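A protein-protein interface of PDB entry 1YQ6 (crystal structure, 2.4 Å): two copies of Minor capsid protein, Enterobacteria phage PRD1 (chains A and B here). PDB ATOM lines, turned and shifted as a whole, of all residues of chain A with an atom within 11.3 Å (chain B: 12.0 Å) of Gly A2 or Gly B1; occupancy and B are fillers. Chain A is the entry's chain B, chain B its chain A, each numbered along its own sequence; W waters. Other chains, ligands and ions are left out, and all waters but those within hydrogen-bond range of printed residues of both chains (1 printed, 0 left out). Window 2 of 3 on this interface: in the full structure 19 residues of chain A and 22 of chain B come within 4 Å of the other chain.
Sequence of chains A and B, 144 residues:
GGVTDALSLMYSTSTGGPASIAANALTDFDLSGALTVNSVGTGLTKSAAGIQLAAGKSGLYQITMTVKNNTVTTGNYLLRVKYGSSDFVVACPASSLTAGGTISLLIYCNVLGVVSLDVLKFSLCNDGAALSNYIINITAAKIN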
ATOM      1  N   GLY A   1     -16.255  -7.258  -6.476  1.00  0.00           N
ATOM      2  CA  GLY A   1     -17.243  -6.108  -6.527  1.00  0.00           C
ATOM      3  C   GLY A   1     -18.317  -6.287  -7.598  1.00  0.00           C
ATOM      4  O   GLY A   1     -19.127  -5.369  -7.858  1.00  0.00           O
ATOM      5  N   GLY A   2     -18.334  -7.460  -8.234  1.00  0.00           N
ATOM      6  CA  GLY A   2     -19.331  -7.705  -9.264  1.00  0.00           C
ATOM      7  C   GLY A   2     -18.922  -7.152 -10.613  1.00  0.00           C
ATOM      8  O   GLY A   2     -17.739  -6.894 -10.871  1.00  0.00           O
ATOM      9  N   VAL A   3     -19.907  -6.973 -11.486  1.00  0.00           N
ATOM     10  CA  VAL A   3     -19.644  -6.457 -12.820  1.00  0.00           C
ATOM     11  C   VAL A   3     -20.384  -5.139 -12.988  1.00  0.00           C
ATOM     12  O   VAL A   3     -21.331  -4.862 -12.248  1.00  0.00           O
ATOM     13  CB  VAL A   3     -20.113  -7.460 -13.890  1.00  0.00           C
ATOM     14  CG1 VAL A   3     -19.400  -8.783 -13.699  1.00  0.00           C
ATOM     15  CG2 VAL A   3     -21.609  -7.655 -13.803  1.00  0.00           C
ATOM     16  N   THR A   4     -19.960  -4.329 -13.953  1.00  0.00           N
ATOM     17  CA  THR A   4     -20.586  -3.035 -14.185  1.00  0.00           C
ATOM     18  C   THR A   4     -21.835  -3.132 -15.046  1.00  0.00           C
ATOM     19  O   THR A   4     -22.776  -2.349 -14.876  1.00  0.00           O
ATOM     20  CB  THR A   4     -19.607  -2.053 -14.857  1.00  0.00           C
ATOM     21  OG1 THR A   4     -19.225  -2.559 -16.143  1.00  0.00           O
ATOM     22  CG2 THR A   4     -18.356  -1.877 -14.002  1.00  0.00           C
ATOM     23  N   ASP A   5     -21.854  -4.086 -15.973  1.00  0.00           N
ATOM     24  CA  ASP A   5     -23.008  -4.248 -16.853  1.00  0.00           C
ATOM     25  C   ASP A   5     -23.335  -5.715 -17.097  1.00  0.00           C
ATOM     26  O   ASP A   5     -22.441  -6.549 -17.190  1.00  0.00           O
ATOM     27  CB  ASP A   5     -22.753  -3.555 -18.195  1.00  0.00           C
ATOM     28  CG  ASP A   5     -22.360  -2.090 -18.037  1.00  0.00           C
ATOM     29  OD1 ASP A   5     -21.203  -1.807 -17.645  1.00  0.00           O
ATOM     30  OD2 ASP A   5     -23.215  -1.216 -18.298  1.00  0.00           O
ATOM     31  N   ALA A   6     -24.618  -6.031 -17.204  1.00  0.00           N
ATOM     32  CA  ALA A   6     -25.026  -7.408 -17.449  1.00  0.00           C
ATOM     33  C   ALA A   6     -26.500  -7.460 -17.792  1.00  0.00           C
ATOM     34  O   ALA A   6     -27.272  -6.619 -17.360  1.00  0.00           O
ATOM     35  CB  ALA A   6     -24.751  -8.262 -16.228  1.00  0.00           C
ATOM     36  N   ASN A  38     -32.698 -10.496 -15.286  1.00  0.00           N
ATOM     37  CA  ASN A  38     -31.833  -9.718 -14.415  1.00  0.00           C
ATOM     38  C   ASN A  38     -31.142  -8.674 -15.263  1.00  0.00           C
ATOM     39  O   ASN A  38     -30.838  -8.908 -16.430  1.00  0.00           O
ATOM     40  CB  ASN A  38     -30.779 -10.605 -13.751  1.00  0.00           C
ATOM     41  CG  ASN A  38     -29.826  -9.816 -12.871  1.00  0.00           C
ATOM     42  OD1 ASN A  38     -30.233  -9.223 -11.879  1.00  0.00           O
ATOM     43  ND2 ASN A  38     -28.552  -9.804 -13.234  1.00  0.00           N
ATOM     44  N   SER A  39     -30.875  -7.524 -14.669  1.00  0.00           N
ATOM     45  CA  SER A  39     -30.247  -6.440 -15.384  1.00  0.00           C
ATOM     46  C   SER A  39     -29.307  -5.672 -14.471  1.00  0.00           C
ATOM     47  O   SER A  39     -29.634  -5.402 -13.321  1.00  0.00           O
ATOM     48  CB  SER A  39     -31.336  -5.513 -15.916  1.00  0.00           C
ATOM     49  OG  SER A  39     -30.794  -4.294 -16.395  1.00  0.00           O
ATOM     50  N   VAL A  40     -28.132  -5.326 -14.976  1.00  0.00           N
ATOM     51  CA  VAL A  40     -27.175  -4.574 -14.185  1.00  0.00           C
ATOM     52  C   VAL A  40     -26.616  -3.452 -15.051  1.00  0.00           C
ATOM     53  O   VAL A  40     -26.126  -3.694 -16.155  1.00  0.00           O
ATOM     54  CB  VAL A  40     -26.016  -5.471 -13.702  1.00  0.00           C
ATOM     55  CG1 VAL A  40     -24.992  -4.642 -12.953  1.00  0.00           C
ATOM     56  CG2 VAL A  40     -26.555  -6.577 -12.807  1.00  0.00           C
ATOM     57  N   GLY A  41     -26.702  -2.221 -14.562  1.00  0.00           N
ATOM     58  CA  GLY A  41     -26.185  -1.094 -15.317  1.00  0.00           C
ATOM     59  C   GLY A  41     -27.043  -0.787 -16.522  1.00  0.00           C
ATOM     60  O   GLY A  41     -28.183  -1.249 -16.621  1.00  0.00           O
ATOM     61  N   LYS A  57     -18.367   1.292 -24.053  1.00  0.00           N
ATOM     62  CA  LYS A  57     -18.349   0.002 -23.366  1.00  0.00           C
ATOM     63  C   LYS A  57     -17.460  -1.095 -23.965  1.00  0.00           C
ATOM     64  O   LYS A  57     -17.798  -2.271 -23.888  1.00  0.00           O
ATOM     65  CB  LYS A  57     -19.777  -0.531 -23.240  1.00  0.00           C
ATOM     66  CG  LYS A  57     -20.664   0.292 -22.319  1.00  0.00           C
ATOM     67  CD  LYS A  57     -20.157   0.252 -20.889  1.00  0.00           C
ATOM     68  CE  LYS A  57     -21.062   1.053 -19.971  1.00  0.00           C
ATOM     69  NZ  LYS A  57     -20.572   1.027 -18.563  1.00  0.00           N
ATOM     70  N   SER A  58     -16.336  -0.728 -24.563  1.00  0.00           N
ATOM     71  CA  SER A  58     -15.445  -1.738 -25.114  1.00  0.00           C
ATOM     72  C   SER A  58     -14.883  -2.554 -23.952  1.00  0.00           C
ATOM     73  O   SER A  58     -14.731  -2.041 -22.840  1.00  0.00           O
ATOM     74  CB  SER A  58     -14.294  -1.085 -25.887  1.00  0.00           C
ATOM     75  OG  SER A  58     -14.746  -0.573 -27.129  1.00  0.00           O
ATOM     76  N   GLY A  59     -14.577  -3.822 -24.202  1.00  0.00           N
ATOM     77  CA  GLY A  59     -14.033  -4.652 -23.144  1.00  0.00           C
ATOM     78  C   GLY A  59     -14.291  -6.138 -23.298  1.00  0.00           C
ATOM     79  O   GLY A  59     -14.650  -6.613 -24.376  1.00  0.00           O
ATOM     80  N   LEU A  60     -14.107  -6.867 -22.203  1.00  0.00           N
ATOM     81  CA  LEU A  60     -14.300  -8.311 -22.172  1.00  0.00           C
ATOM     82  C   LEU A  60     -15.725  -8.689 -21.762  1.00  0.00           C
ATOM     83  O   LEU A  60     -16.248  -8.218 -20.750  1.00  0.00           O
ATOM     84  CB  LEU A  60     -13.280  -8.936 -21.217  1.00  0.00           C
ATOM     85  CG  LEU A  60     -11.834  -8.870 -21.722  1.00  0.00           C
ATOM     86  CD1 LEU A  60     -10.867  -9.163 -20.603  1.00  0.00           C
ATOM     87  CD2 LEU A  60     -11.658  -9.857 -22.861  1.00  0.00           C
ATOM     88  N   GLN A  62     -18.601 -11.888 -21.108  1.00  0.00           N
ATOM     89  CA  GLN A  62     -18.877 -13.297 -20.867  1.00  0.00           C
ATOM     90  C   GLN A  62     -20.301 -13.502 -21.373  1.00  0.00           C
ATOM     91  O   GLN A  62     -21.226 -12.809 -20.954  1.00  0.00           O
ATOM     92  CB  GLN A  62     -18.770 -13.614 -19.372  1.00  0.00           C
ATOM     93  CG  GLN A  62     -19.041 -15.077 -19.010  1.00  0.00           C
ATOM     94  CD  GLN A  62     -18.181 -16.047 -19.809  1.00  0.00           C
ATOM     95  OE1 GLN A  62     -16.954 -15.955 -19.798  1.00  0.00           O
ATOM     96  NE2 GLN A  62     -18.826 -16.982 -20.510  1.00  0.00           N
ATOM     97  N   ALA A 140     -25.360 -11.979 -20.794  1.00  0.00           N
ATOM     98  CA  ALA A 140     -24.112 -11.346 -21.178  1.00  0.00           C
ATOM     99  C   ALA A 140     -23.689 -10.450 -20.037  1.00  0.00           C
ATOM    100  O   ALA A 140     -24.513  -9.783 -19.424  1.00  0.00           O
ATOM    101  CB  ALA A 140     -24.293 -10.535 -22.449  1.00  0.00           C
ATOM    102  N   ALA A 141     -22.403 -10.450 -19.735  1.00  0.00           N
ATOM    103  CA  ALA A 141     -21.890  -9.626 -18.661  1.00  0.00           C
ATOM    104  C   ALA A 141     -20.532  -9.090 -19.057  1.00  0.00           C
ATOM    105  O   ALA A 141     -19.700  -9.813 -19.604  1.00  0.00           O
ATOM    106  CB  ALA A 141     -21.776 -10.437 -17.381  1.00  0.00           C
ATOM    107  N   LYS A 142     -20.316  -7.810 -18.789  1.00  0.00           N
ATOM    108  CA  LYS A 142     -19.048  -7.161 -19.077  1.00  0.00           C
ATOM    109  C   LYS A 142     -18.167  -7.428 -17.855  1.00  0.00           C
ATOM    110  O   LYS A 142     -18.472  -6.947 -16.768  1.00  0.00           O
ATOM    111  CB  LYS A 142     -19.279  -5.658 -19.246  1.00  0.00           C
ATOM    112  CG  LYS A 142     -18.059  -4.848 -19.653  1.00  0.00           C
ATOM    113  CD  LYS A 142     -18.438  -3.384 -19.865  1.00  0.00           C
ATOM    114  CE  LYS A 142     -17.291  -2.584 -20.444  1.00  0.00           C
ATOM    115  NZ  LYS A 142     -16.109  -2.601 -19.554  1.00  0.00           N
ATOM    116  N   ILE A 143     -17.090  -8.194 -18.009  1.00  0.00           N
ATOM    117  CA  ILE A 143     -16.252  -8.473 -16.852  1.00  0.00           C
ATOM    118  C   ILE A 143     -15.008  -7.599 -16.755  1.00  0.00           C
ATOM    119  O   ILE A 143     -14.246  -7.699 -15.796  1.00  0.00           O
ATOM    120  CB  ILE A 143     -15.840  -9.961 -16.784  1.00  0.00           C
ATOM    121  CG1 ILE A 143     -14.848 -10.283 -17.886  1.00  0.00           C
ATOM    122  CG2 ILE A 143     -17.072 -10.848 -16.900  1.00  0.00           C
ATOM    123  CD1 ILE A 143     -14.138 -11.586 -17.653  1.00  0.00           C
ATOM    124  N   ASN A 144     -14.802  -6.745 -17.755  1.00  0.00           N
ATOM    125  CA  ASN A 144     -13.676  -5.814 -17.757  1.00  0.00           C
ATOM    126  C   ASN A 144     -13.881  -4.734 -18.812  1.00  0.00           C
ATOM    127  O   ASN A 144     -13.413  -3.594 -18.596  1.00  0.00           O
ATOM    128  CB  ASN A 144     -12.350  -6.518 -18.022  1.00  0.00           C
ATOM    129  CG  ASN A 144     -11.153  -5.633 -17.685  1.00  0.00           C
ATOM    130  OD1 ASN A 144     -10.897  -5.339 -16.514  1.00  0.00           O
ATOM    131  ND2 ASN A 144     -10.424  -5.195 -18.711  1.00  0.00           N
ATOM    132  OXT ASN A 144     -14.492  -5.050 -19.854  1.00  0.00           O
ATOM    133  N   GLY B   1     -15.141  -3.929 -10.865  1.00  0.00           N
ATOM    134  CA  GLY B   1     -13.783  -3.281 -11.075  1.00  0.00           C
ATOM    135  C   GLY B   1     -12.949  -3.956 -12.166  1.00  0.00           C
ATOM    136  O   GLY B   1     -11.766  -3.608 -12.384  1.00  0.00           O
ATOM    137  N   GLY B   2     -13.552  -4.922 -12.859  1.00  0.00           N
ATOM    138  CA  GLY B   2     -12.833  -5.608 -13.919  1.00  0.00           C
ATOM    139  C   GLY B   2     -11.956  -6.726 -13.391  1.00  0.00           C
ATOM    140  O   GLY B   2     -12.156  -7.224 -12.276  1.00  0.00           O
ATOM    141  N   VAL B   3     -10.976  -7.123 -14.198  1.00  0.00           N
ATOM    142  CA  VAL B   3     -10.073  -8.194 -13.815  1.00  0.00           C
ATOM    143  C   VAL B   3      -8.660  -7.639 -13.747  1.00  0.00           C
ATOM    144  O   VAL B   3      -8.378  -6.590 -14.331  1.00  0.00           O
ATOM    145  CB  VAL B   3     -10.141  -9.345 -14.834  1.00  0.00           C
ATOM    146  CG1 VAL B   3     -11.552  -9.858 -14.927  1.00  0.00           C
ATOM    147  CG2 VAL B   3      -9.662  -8.870 -16.193  1.00  0.00           C
ATOM    148  N   THR B   4      -7.778  -8.333 -13.031  1.00  0.00           N
ATOM    149  CA  THR B   4      -6.397  -7.886 -12.896  1.00  0.00           C
ATOM    150  C   THR B   4      -5.523  -8.291 -14.075  1.00  0.00           C
ATOM    151  O   THR B   4      -4.596  -7.574 -14.434  1.00  0.00           O
ATOM    152  CB  THR B   4      -5.755  -8.437 -11.608  1.00  0.00           C
ATOM    153  OG1 THR B   4      -5.704  -9.870 -11.664  1.00  0.00           O
ATOM    154  CG2 THR B   4      -6.560  -8.004 -10.393  1.00  0.00           C
ATOM    155  N   ASP B   5      -5.811  -9.438 -14.681  1.00  0.00           N
ATOM    156  CA  ASP B   5      -5.017  -9.910 -15.811  1.00  0.00           C
ATOM    157  C   ASP B   5      -5.882 -10.548 -16.886  1.00  0.00           C
ATOM    158  O   ASP B   5      -6.873 -11.220 -16.587  1.00  0.00           O
ATOM    159  CB  ASP B   5      -3.972 -10.929 -15.338  1.00  0.00           C
ATOM    160  CG  ASP B   5      -3.096 -10.397 -14.214  1.00  0.00           C
ATOM    161  OD1 ASP B   5      -3.563 -10.318 -13.059  1.00  0.00           O
ATOM    162  OD2 ASP B   5      -1.932 -10.055 -14.485  1.00  0.00           O
ATOM    163  N   ALA B   6      -5.509 -10.344 -18.143  1.00  0.00           N
ATOM    164  CA  ALA B   6      -6.267 -10.920 -19.243  1.00  0.00           C
ATOM    165  C   ALA B   6      -5.495 -10.782 -20.537  1.00  0.00           C
ATOM    166  O   ALA B   6      -4.703  -9.863 -20.700  1.00  0.00           O
ATOM    167  CB  ALA B   6      -7.616 -10.233 -19.367  1.00  0.00           C
ATOM    168  N   ASN B  38      -6.286  -7.722 -27.162  1.00  0.00           N
ATOM    169  CA  ASN B  38      -6.475  -6.949 -25.947  1.00  0.00           C
ATOM    170  C   ASN B  38      -5.584  -7.539 -24.883  1.00  0.00           C
ATOM    171  O   ASN B  38      -5.359  -8.748 -24.847  1.00  0.00           O
ATOM    172  CB  ASN B  38      -7.927  -7.005 -25.482  1.00  0.00           C
ATOM    173  CG  ASN B  38      -8.150  -6.238 -24.192  1.00  0.00           C
ATOM    174  OD1 ASN B  38      -7.982  -5.022 -24.147  1.00  0.00           O
ATOM    175  ND2 ASN B  38      -8.521  -6.949 -23.133  1.00  0.00           N
ATOM    176  N   SER B  39      -5.092  -6.687 -24.000  1.00  0.00           N
ATOM    177  CA  SER B  39      -4.195  -7.125 -22.954  1.00  0.00           C
ATOM    178  C   SER B  39      -4.449  -6.341 -21.676  1.00  0.00           C
ATOM    179  O   SER B  39      -4.643  -5.134 -21.715  1.00  0.00           O
ATOM    180  CB  SER B  39      -2.759  -6.912 -23.437  1.00  0.00           C
ATOM    181  OG  SER B  39      -1.823  -7.072 -22.394  1.00  0.00           O
ATOM    182  N   VAL B  40      -4.461  -7.030 -20.544  1.00  0.00           N
ATOM    183  CA  VAL B  40      -4.679  -6.378 -19.264  1.00  0.00           C
ATOM    184  C   VAL B  40      -3.663  -6.915 -18.268  1.00  0.00           C
ATOM    185  O   VAL B  40      -3.553  -8.124 -18.080  1.00  0.00           O
ATOM    186  CB  VAL B  40      -6.107  -6.639 -18.729  1.00  0.00           C
ATOM    187  CG1 VAL B  40      -6.275  -5.997 -17.358  1.00  0.00           C
ATOM    188  CG2 VAL B  40      -7.137  -6.067 -19.684  1.00  0.00           C
ATOM    189  N   GLY B  41      -2.912  -6.017 -17.642  1.00  0.00           N
ATOM    190  CA  GLY B  41      -1.920  -6.443 -16.674  1.00  0.00           C
ATOM    191  C   GLY B  41      -0.741  -7.121 -17.333  1.00  0.00           C
ATOM    192  O   GLY B  41      -0.554  -7.005 -18.542  1.00  0.00           O
ATOM    193  N   ALA B 141      -8.724 -14.828 -18.867  1.00  0.00           N
ATOM    194  CA  ALA B 141      -8.817 -13.754 -17.898  1.00  0.00           C
ATOM    195  C   ALA B 141      -8.819 -14.337 -16.495  1.00  0.00           C
ATOM    196  O   ALA B 141      -9.492 -15.331 -16.224  1.00  0.00           O
ATOM    197  CB  ALA B 141     -10.074 -12.955 -18.128  1.00  0.00           C
ATOM    198  N   LYS B 142      -8.044 -13.717 -15.613  1.00  0.00           N
ATOM    199  CA  LYS B 142      -7.963 -14.135 -14.223  1.00  0.00           C
ATOM    200  C   LYS B 142      -9.131 -13.429 -13.528  1.00  0.00           C
ATOM    201  O   LYS B 142      -9.147 -12.203 -13.452  1.00  0.00           O
ATOM    202  CB  LYS B 142      -6.623 -13.674 -13.635  1.00  0.00           C
ATOM    203  CG  LYS B 142      -6.343 -14.124 -12.210  1.00  0.00           C
ATOM    204  CD  LYS B 142      -4.957 -13.683 -11.769  1.00  0.00           C
ATOM    205  CE  LYS B 142      -4.584 -14.267 -10.418  1.00  0.00           C
ATOM    206  NZ  LYS B 142      -5.542 -13.865  -9.363  1.00  0.00           N
ATOM    207  N   ILE B 143     -10.118 -14.172 -13.038  1.00  0.00           N
ATOM    208  CA  ILE B 143     -11.243 -13.511 -12.386  1.00  0.00           C
ATOM    209  C   ILE B 143     -11.160 -13.512 -10.861  1.00  0.00           C
ATOM    210  O   ILE B 143     -12.018 -12.944 -10.195  1.00  0.00           O
ATOM    211  CB  ILE B 143     -12.601 -14.109 -12.825  1.00  0.00           C
ATOM    212  CG1 ILE B 143     -12.773 -15.505 -12.257  1.00  0.00           C
ATOM    213  CG2 ILE B 143     -12.683 -14.149 -14.344  1.00  0.00           C
ATOM    214  CD1 ILE B 143     -14.200 -15.988 -12.332  1.00  0.00           C
ATOM    215  N   ASN B 144     -10.132 -14.154 -10.317  1.00  0.00           N
ATOM    216  CA  ASN B 144      -9.904 -14.181  -8.871  1.00  0.00           C
ATOM    217  C   ASN B 144      -8.501 -14.661  -8.556  1.00  0.00           C
ATOM    218  O   ASN B 144      -7.938 -14.209  -7.537  1.00  0.00           O
ATOM    219  CB  ASN B 144     -10.903 -15.077  -8.146  1.00  0.00           C
ATOM    220  CG  ASN B 144     -10.906 -14.833  -6.644  1.00  0.00           C
ATOM    221  OD1 ASN B 144     -11.351 -13.779  -6.183  1.00  0.00           O
ATOM    222  ND2 ASN B 144     -10.401 -15.797  -5.877  1.00  0.00           N
ATOM    223  OXT ASN B 144      -7.992 -15.507  -9.319  1.00  0.00           O
HETATM  224  O   HOH W   1     -10.628  -5.680 -21.462  1.00  0.00           O
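The backbone NH (N) of Val B3 is in hydrogen-bond range of the side-chain amide oxygen (OD1) of Asn A144, 2.9 Å away.
The backbone carbonyl oxygen of Ala B6 sits at hydrogen-bond distance from the backbone NH of Val B40 (2.8 Å).
N of Ile A143 lies within hydrogen-bond range of O of Leu A60, 2.9 Å away.
The chain-end carboxylate (OXT) of Asn A144 lies within hydrogen-bond range of the backbone NH (N) of Leu A60 (3.0 Å).
The side-chain amino group (NZ) of Lys A142 is in salt-bridge range of the chain-end carboxylate (OXT) of Asn A144 (2.9 Å).
Among the printed residues, pairs that only touch across the chains: Ile A143 with Gly B2, Asn A144 with Gly B2, Asn A144 with Val B40, Ile A143 with Val B3, Leu A60 with Ala B6 and Gly A2 with Gly B1.
No residue of chain B comes within 4 Å of Gly A1.
Of chain B, only Gly B1 (3.9 Å) comes within 4 Å of Gly A2.
No residue of chain B comes within 4 Å of Val A3.
No residue of chain B comes within 4 Å of Thr A4.
Of the printed residues of chain B, Ile A143 touches Gly B2 (3.1 Å) and Val B3 (3.6 Å).
Gly B1 touches just one residue of chain A: Gly A2.
Of chain A, only Ile A143 (3.1 Å) and Asn A144 (3.2 Å) come within 4 Å of Gly B2.
Printed residues of chain A within 4 Å of Val B40: Asn A144 (3.5 Å).
The nearest residue of chain A that does not touch Gly B1 is Asn A144 (4.6 Å).
Of the 14 printed residues of chain B, 5 touch a printed residue of chain A.
Printed residues of chain B that touch a printed residue of chain A: Gly B1, Gly B2, Val B3, Ala B6 and Val B40.
Of the 20 printed residues of chain A, 4 touch a printed residue of chain B.
Printed residues of chain A that touch a printed residue of chain B: Gly A2, Leu A60, Ile A143 and Asn A144.
Hydrophobic or aromatic side chains of chain A that line the printed part of chain B: Leu A60.
Among the printed residues, 7 pairs touch across the chains.
Among the printed residues, no Asp or Glu carboxylate lies within 4 Å of a Lys or Arg side-chain nitrogen of the other chain.
Ile A143 touches Gly B2, but with the chains exchanged Gly A2 does not touch Ile B143 (8.4 Å).
Asn A144 touches Gly B2, but with the chains exchanged Gly A2 does not touch Asn B144 (9.6 Å).
Asn A144 touches Val B3, but with the chains exchanged Val A3 does not touch Asn B144 (11.2 Å).
Asn A144 touches Val B40, but with the chains exchanged Val A40 does not touch Asn B144 (17.8 Å).
Of the 7 pairs that touch across the chains among the printed residues, none has its exchanged pair printed and touching as well.
Water W1 bridges the side-chain amide nitrogen (ND2) of Asn A144 (2.8 Å) and the side-chain amide nitrogen (ND2) of Asn B38 (3.0 Å).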
